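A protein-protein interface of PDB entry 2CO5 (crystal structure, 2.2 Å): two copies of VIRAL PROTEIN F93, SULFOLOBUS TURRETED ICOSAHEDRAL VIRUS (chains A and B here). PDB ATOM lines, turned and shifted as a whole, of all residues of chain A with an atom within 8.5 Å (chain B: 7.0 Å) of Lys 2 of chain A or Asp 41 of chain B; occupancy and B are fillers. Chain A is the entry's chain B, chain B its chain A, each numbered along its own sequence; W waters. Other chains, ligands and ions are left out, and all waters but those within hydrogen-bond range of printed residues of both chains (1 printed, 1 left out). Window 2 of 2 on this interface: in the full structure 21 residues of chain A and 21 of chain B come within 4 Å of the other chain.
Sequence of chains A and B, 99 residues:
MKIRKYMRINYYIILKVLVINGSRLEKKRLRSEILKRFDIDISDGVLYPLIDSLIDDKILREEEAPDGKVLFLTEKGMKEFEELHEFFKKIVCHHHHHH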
ATOM      1  N   MET A   1      -0.833  15.721  -8.632  1.00  0.00           N
ATOM      2  CA  MET A   1       0.424  15.386  -9.342  1.00  0.00           C
ATOM      3  C   MET A   1       1.099  14.208  -8.636  1.00  0.00           C
ATOM      4  O   MET A   1       1.114  14.143  -7.413  1.00  0.00           O
ATOM      5  CB  MET A   1       1.356  16.600  -9.353  1.00  0.00           C
ATOM      6  CG  MET A   1       2.451  16.523 -10.402  1.00  0.00           C
ATOM      7  SD  MET A   1       3.686  17.839 -10.306  1.00  0.00           S
ATOM      8  CE  MET A   1       3.724  18.230  -8.562  1.00  0.00           C
ATOM      9  N   LYS A   2       1.630  13.273  -9.414  1.00  0.00           N
ATOM     10  CA  LYS A   2       2.411  12.163  -8.873  1.00  0.00           C
ATOM     11  C   LYS A   2       3.890  12.451  -9.058  1.00  0.00           C
ATOM     12  O   LYS A   2       4.277  13.224  -9.930  1.00  0.00           O
ATOM     13  CB  LYS A   2       2.054  10.846  -9.570  1.00  0.00           C
ATOM     14  CG  LYS A   2       0.656  10.336  -9.260  1.00  0.00           C
ATOM     15  CD  LYS A   2       0.387   9.022  -9.960  1.00  0.00           C
ATOM     16  CE  LYS A   2      -1.082   8.638  -9.860  1.00  0.00           C
ATOM     17  NZ  LYS A   2      -1.511   8.437  -8.443  1.00  0.00           N
ATOM     18  N   ILE A   3       4.710  11.825  -8.222  1.00  0.00           N
ATOM     19  CA  ILE A   3       6.156  11.941  -8.331  1.00  0.00           C
ATOM     20  C   ILE A   3       6.585  11.220  -9.595  1.00  0.00           C
ATOM     21  O   ILE A   3       6.177  10.084  -9.825  1.00  0.00           O
ATOM     22  CB  ILE A   3       6.868  11.315  -7.118  1.00  0.00           C
ATOM     23  CG1 ILE A   3       6.496  12.066  -5.831  1.00  0.00           C
ATOM     24  CG2 ILE A   3       8.388  11.300  -7.332  1.00  0.00           C
ATOM     25  CD1 ILE A   3       6.928  13.500  -5.807  1.00  0.00           C
ATOM     26  N   ARG A   4       7.400  11.885 -10.410  1.00  0.00           N
ATOM     27  CA  ARG A   4       7.844  11.320 -11.682  1.00  0.00           C
ATOM     28  C   ARG A   4       9.358  11.144 -11.685  1.00  0.00           C
ATOM     29  O   ARG A   4      10.058  11.734 -10.859  1.00  0.00           O
ATOM     30  CB  ARG A   4       7.368  12.200 -12.841  1.00  0.00           C
ATOM     31  CG  ARG A   4       5.841  12.247 -12.950  1.00  0.00           C
ATOM     32  CD  ARG A   4       5.355  13.108 -14.110  1.00  0.00           C
ATOM     33  NE  ARG A   4       5.581  12.475 -15.409  1.00  0.00           N
ATOM     34  CZ  ARG A   4       4.848  11.485 -15.919  1.00  0.00           C
ATOM     35  NH1 ARG A   4       3.817  10.976 -15.248  1.00  0.00           N
ATOM     36  NH2 ARG A   4       5.153  10.995 -17.114  1.00  0.00           N
ATOM     37  N   LYS A   5       9.851  10.327 -12.616  1.00  0.00           N
ATOM     38  CA  LYS A   5      11.248   9.850 -12.600  1.00  0.00           C
ATOM     39  C   LYS A   5      12.332  10.922 -12.560  1.00  0.00           C
ATOM     40  O   LYS A   5      13.387  10.709 -11.966  1.00  0.00           O
ATOM     41  CB  LYS A   5      11.517   8.892 -13.774  1.00  0.00           C
ATOM     42  CG  LYS A   5      11.504   9.524 -15.162  1.00  0.00           C
ATOM     43  CD  LYS A   5      11.693   8.473 -16.256  1.00  0.00           C
ATOM     44  CE  LYS A   5      11.258   9.002 -17.617  1.00  0.00           C
ATOM     45  NZ  LYS A   5      11.488   8.032 -18.725  1.00  0.00           N
ATOM     46  N   MET A   7      12.191  13.737 -11.001  1.00  0.00           N
ATOM     47  CA  MET A   7      12.094  14.522  -9.771  1.00  0.00           C
ATOM     48  C   MET A   7      13.174  14.078  -8.797  1.00  0.00           C
ATOM     49  O   MET A   7      12.908  13.540  -7.727  1.00  0.00           O
ATOM     50  CB  MET A   7      10.688  14.444  -9.173  1.00  0.00           C
ATOM     51  CG  MET A   7       9.653  15.037 -10.122  1.00  0.00           C
ATOM     52  SD  MET A   7       7.958  15.039  -9.544  1.00  0.00           S
ATOM     53  CE  MET A   7       7.155  15.901 -10.898  1.00  0.00           C
ATOM     54  N   GLU A  83       8.754  22.144 -15.814  1.00  0.00           N
ATOM     55  CA  GLU A  83       7.982  21.296 -14.908  1.00  0.00           C
ATOM     56  C   GLU A  83       8.741  20.990 -13.613  1.00  0.00           C
ATOM     57  O   GLU A  83       8.185  21.109 -12.522  1.00  0.00           O
ATOM     58  CB  GLU A  83       7.585  19.987 -15.590  1.00  0.00           C
ATOM     59  CG  GLU A  83       6.576  20.158 -16.712  1.00  0.00           C
ATOM     60  CD  GLU A  83       6.053  18.832 -17.228  1.00  0.00           C
ATOM     61  OE1 GLU A  83       5.559  18.027 -16.403  1.00  0.00           O
ATOM     62  OE2 GLU A  83       6.131  18.599 -18.457  1.00  0.00           O
ATOM     63  N   PHE A  87       7.986  22.231  -9.762  1.00  0.00           N
ATOM     64  CA  PHE A  87       7.819  21.209  -8.731  1.00  0.00           C
ATOM     65  C   PHE A  87       8.711  21.494  -7.507  1.00  0.00           C
ATOM     66  O   PHE A  87       8.217  21.576  -6.376  1.00  0.00           O
ATOM     67  CB  PHE A  87       8.116  19.816  -9.294  1.00  0.00           C
ATOM     68  CG  PHE A  87       8.274  18.768  -8.230  1.00  0.00           C
ATOM     69  CD1 PHE A  87       7.157  18.205  -7.624  1.00  0.00           C
ATOM     70  CD2 PHE A  87       9.536  18.371  -7.810  1.00  0.00           C
ATOM     71  CE1 PHE A  87       7.296  17.249  -6.630  1.00  0.00           C
ATOM     72  CE2 PHE A  87       9.686  17.417  -6.823  1.00  0.00           C
ATOM     73  CZ  PHE A  87       8.562  16.854  -6.229  1.00  0.00           C
ATOM     74  N   LYS A  90       7.834  24.613  -5.543  1.00  0.00           N
ATOM     75  CA  LYS A  90       6.639  24.362  -4.736  1.00  0.00           C
ATOM     76  C   LYS A  90       6.934  23.602  -3.441  1.00  0.00           C
ATOM     77  O   LYS A  90       6.373  23.928  -2.400  1.00  0.00           O
ATOM     78  CB  LYS A  90       5.578  23.609  -5.558  1.00  0.00           C
ATOM     79  CG  LYS A  90       4.337  23.187  -4.776  1.00  0.00           C
ATOM     80  CD  LYS A  90       3.244  22.619  -5.692  1.00  0.00           C
ATOM     81  CE  LYS A  90       3.671  21.300  -6.339  1.00  0.00           C
ATOM     82  NZ  LYS A  90       2.527  20.567  -6.955  1.00  0.00           N
ATOM     83  N   ASN B  10      10.510  11.625  -1.812  1.00  0.00           N
ATOM     84  CA  ASN B  10       9.414  11.174  -0.938  1.00  0.00           C
ATOM     85  C   ASN B  10       9.758  11.375   0.537  1.00  0.00           C
ATOM     86  O   ASN B  10       8.933  11.816   1.335  1.00  0.00           O
ATOM     87  CB  ASN B  10       9.101   9.693  -1.169  1.00  0.00           C
ATOM     88  CG  ASN B  10       8.468   9.425  -2.520  1.00  0.00           C
ATOM     89  OD1 ASN B  10       7.320   9.778  -2.760  1.00  0.00           O
ATOM     90  ND2 ASN B  10       9.211   8.774  -3.401  1.00  0.00           N
ATOM     91  N   ARG B  31      -1.154  11.076   3.889  1.00  0.00           N
ATOM     92  CA  ARG B  31      -1.437  11.081   2.468  1.00  0.00           C
ATOM     93  C   ARG B  31      -2.281  12.284   2.053  1.00  0.00           C
ATOM     94  O   ARG B  31      -1.951  12.965   1.079  1.00  0.00           O
ATOM     95  CB  ARG B  31      -2.150   9.791   2.066  1.00  0.00           C
ATOM     96  CG  ARG B  31      -2.189   9.622   0.584  1.00  0.00           C
ATOM     97  CD  ARG B  31      -2.929   8.387   0.130  1.00  0.00           C
ATOM     98  NE  ARG B  31      -3.266   8.549  -1.281  1.00  0.00           N
ATOM     99  CZ  ARG B  31      -3.507   7.561  -2.130  1.00  0.00           C
ATOM    100  NH1 ARG B  31      -3.460   6.294  -1.734  1.00  0.00           N
ATOM    101  NH2 ARG B  31      -3.797   7.850  -3.394  1.00  0.00           N
ATOM    102  N   ILE B  34      -0.252  15.675   2.425  1.00  0.00           N
ATOM    103  CA  ILE B  34       0.668  15.873   1.306  1.00  0.00           C
ATOM    104  C   ILE B  34      -0.073  16.404   0.071  1.00  0.00           C
ATOM    105  O   ILE B  34       0.419  17.296  -0.625  1.00  0.00           O
ATOM    106  CB  ILE B  34       1.406  14.567   0.955  1.00  0.00           C
ATOM    107  CG1 ILE B  34       2.403  14.209   2.062  1.00  0.00           C
ATOM    108  CG2 ILE B  34       2.142  14.698  -0.372  1.00  0.00           C
ATOM    109  CD1 ILE B  34       2.899  12.796   2.012  1.00  0.00           C
ATOM    110  N   LEU B  35      -1.256  15.852  -0.179  1.00  0.00           N
ATOM    111  CA  LEU B  35      -2.094  16.246  -1.312  1.00  0.00           C
ATOM    112  C   LEU B  35      -2.634  17.671  -1.097  1.00  0.00           C
ATOM    113  O   LEU B  35      -2.649  18.479  -2.021  1.00  0.00           O
ATOM    114  CB  LEU B  35      -3.256  15.257  -1.482  1.00  0.00           C
ATOM    115  CG  LEU B  35      -3.561  14.673  -2.867  1.00  0.00           C
ATOM    116  CD1 LEU B  35      -4.825  13.802  -2.780  1.00  0.00           C
ATOM    117  CD2 LEU B  35      -3.728  15.734  -3.936  1.00  0.00           C
ATOM    118  N   PHE B  38       0.709  20.238  -0.981  1.00  0.00           N
ATOM    119  CA  PHE B  38       1.556  20.296  -2.186  1.00  0.00           C
ATOM    120  C   PHE B  38       0.909  19.787  -3.477  1.00  0.00           C
ATOM    121  O   PHE B  38       1.567  19.773  -4.515  1.00  0.00           O
ATOM    122  CB  PHE B  38       2.842  19.510  -1.947  1.00  0.00           C
ATOM    123  CG  PHE B  38       3.611  19.968  -0.747  1.00  0.00           C
ATOM    124  CD1 PHE B  38       4.117  21.261  -0.692  1.00  0.00           C
ATOM    125  CD2 PHE B  38       3.836  19.112   0.327  1.00  0.00           C
ATOM    126  CE1 PHE B  38       4.833  21.700   0.414  1.00  0.00           C
ATOM    127  CE2 PHE B  38       4.551  19.544   1.440  1.00  0.00           C
ATOM    128  CZ  PHE B  38       5.048  20.841   1.481  1.00  0.00           C
ATOM    129  N   ASP B  39      -0.362  19.384  -3.428  1.00  0.00           N
ATOM    130  CA  ASP B  39      -1.014  18.762  -4.579  1.00  0.00           C
ATOM    131  C   ASP B  39      -0.150  17.625  -5.144  1.00  0.00           C
ATOM    132  O   ASP B  39       0.022  17.491  -6.359  1.00  0.00           O
ATOM    133  CB  ASP B  39      -1.326  19.815  -5.654  1.00  0.00           C
ATOM    134  CG  ASP B  39      -2.309  19.315  -6.712  1.00  0.00           C
ATOM    135  OD1 ASP B  39      -3.138  18.427  -6.404  1.00  0.00           O
ATOM    136  OD2 ASP B  39      -2.248  19.814  -7.858  1.00  0.00           O
ATOM    137  N   ILE B  40       0.410  16.821  -4.242  1.00  0.00           N
ATOM    138  CA  ILE B  40       1.186  15.657  -4.626  1.00  0.00           C
ATOM    139  C   ILE B  40       0.487  14.409  -4.105  1.00  0.00           C
ATOM    140  O   ILE B  40       0.144  14.316  -2.925  1.00  0.00           O
ATOM    141  CB  ILE B  40       2.648  15.727  -4.130  1.00  0.00           C
ATOM    142  CG1 ILE B  40       3.379  16.879  -4.830  1.00  0.00           C
ATOM    143  CG2 ILE B  40       3.388  14.415  -4.421  1.00  0.00           C
ATOM    144  CD1 ILE B  40       4.592  17.360  -4.091  1.00  0.00           C
ATOM    145  N   ASP B  41       0.268  13.471  -5.019  1.00  0.00           N
ATOM    146  CA  ASP B  41      -0.379  12.211  -4.732  1.00  0.00           C
ATOM    147  C   ASP B  41       0.691  11.140  -4.539  1.00  0.00           C
ATOM    148  O   ASP B  41       1.342  10.736  -5.504  1.00  0.00           O
ATOM    149  CB  ASP B  41      -1.296  11.853  -5.902  1.00  0.00           C
ATOM    150  CG  ASP B  41      -1.965  10.501  -5.743  1.00  0.00           C
ATOM    151  OD1 ASP B  41      -1.720   9.813  -4.732  1.00  0.00           O
ATOM    152  OD2 ASP B  41      -2.738  10.124  -6.650  1.00  0.00           O
ATOM    153  N   ILE B  42       0.875  10.693  -3.296  1.00  0.00           N
ATOM    154  CA  ILE B  42       1.806   9.603  -2.994  1.00  0.00           C
ATOM    155  C   ILE B  42       1.015   8.421  -2.433  1.00  0.00           C
ATOM    156  O   ILE B  42       0.170   8.580  -1.549  1.00  0.00           O
ATOM    157  CB  ILE B  42       2.926  10.035  -2.004  1.00  0.00           C
ATOM    158  CG1 ILE B  42       3.721  11.221  -2.553  1.00  0.00           C
ATOM    159  CG2 ILE B  42       3.891   8.883  -1.738  1.00  0.00           C
ATOM    160  CD1 ILE B  42       4.853  11.702  -1.611  1.00  0.00           C
ATOM    161  N   SER B  43       1.295   7.238  -2.968  1.00  0.00           N
ATOM    162  CA  SER B  43       0.616   6.002  -2.579  1.00  0.00           C
ATOM    163  C   SER B  43       0.939   5.579  -1.144  1.00  0.00           C
ATOM    164  O   SER B  43       2.038   5.819  -0.661  1.00  0.00           O
ATOM    165  CB  SER B  43       1.045   4.876  -3.528  1.00  0.00           C
ATOM    166  OG  SER B  43       0.466   3.637  -3.152  1.00  0.00           O
ATOM    167  N   ASP B  44      -0.019   4.933  -0.483  1.00  0.00           N
ATOM    168  CA  ASP B  44       0.219   4.241   0.794  1.00  0.00           C
ATOM    169  C   ASP B  44       1.276   3.155   0.636  1.00  0.00           C
ATOM    170  O   ASP B  44       1.988   2.831   1.582  1.00  0.00           O
ATOM    171  CB  ASP B  44      -1.066   3.568   1.304  1.00  0.00           C
ATOM    172  CG  ASP B  44      -2.101   4.561   1.811  1.00  0.00           C
ATOM    173  OD1 ASP B  44      -1.705   5.581   2.412  1.00  0.00           O
ATOM    174  OD2 ASP B  44      -3.315   4.300   1.622  1.00  0.00           O
HETATM  175  O   HOH W   1       3.706   9.906  -6.307  1.00  0.00           O
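Water W1 bridges O of Asp 41 of chain B and N of Ile 3 of chain A.
The side-chain carboxylate (OD2) of Asp 41 of chain B is in salt-bridge range of the side-chain amino group (NZ) of Lys 2 of chain A, at 2.8 Å.
The backbone carbonyl oxygen of Phe 38 of chain B lies within hydrogen-bond range of the side-chain amino group of Lys 90 of chain A, at 2.7 Å.
The backbone NH (N) of Met 1 of chain A sits at hydrogen-bond distance from the backbone carbonyl oxygen (O) of Asp 39 of chain B, 3.0 Å away.
N of Asp 41 of chain B sits at hydrogen-bond distance from O of Met 1 of chain A (2.6 Å).
Printed residues of chain A within 4 Å of Ile 40 of chain B: Met 1 (3.2 Å), Ile 3 (3.9 Å) and Phe 87 (3.7 Å).
Of the printed residues of chain B, Phe 87 of chain A touches Ile 40.
Printed residues of chain A within 4 Å of Asp 39 of chain B: Met 1 (3.0 Å).
Of the printed residues of chain B, Ile 3 of chain A touches Asn 10 and Ile 40.
The side-chain carboxylate of Asp 41 of chain B lies within salt-bridge range of the guanidinium group of Arg 31 of chain B (3.2 Å).
O of Ile 40 of chain B sits close to N of Leu 35 of chain B (3.4 Å).
Of the 9 printed residues of chain A, 5 touch a printed residue of chain B.
Hydrophobic or aromatic side chains of chain A that line the printed part of chain B: Met 1, Ile 3 and Phe 87.
Of the 11 printed residues of chain B, 5 touch a printed residue of chain A.
Hydrophobic or aromatic side chains of chain B that line the printed part of chain A: Phe 38 and Ile 40.
No position is printed for both chains.
Of the 8 pairs that touch across the chains among the printed residues, none has its exchanged pair printed and touching as well.
Met 1 of chain A touches Ile 40 of chain B (O to CA, 3.2 Å).
Ile 3 of chain A touches Asn 10 of chain B (CG1 to OD1, 3.9 Å).
Ile 3 of chain A touches Ile 40 of chain B.
CE1 of Phe 87 of chain A touches CD1 of Ile 40 of chain B, at 3.7 Å.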
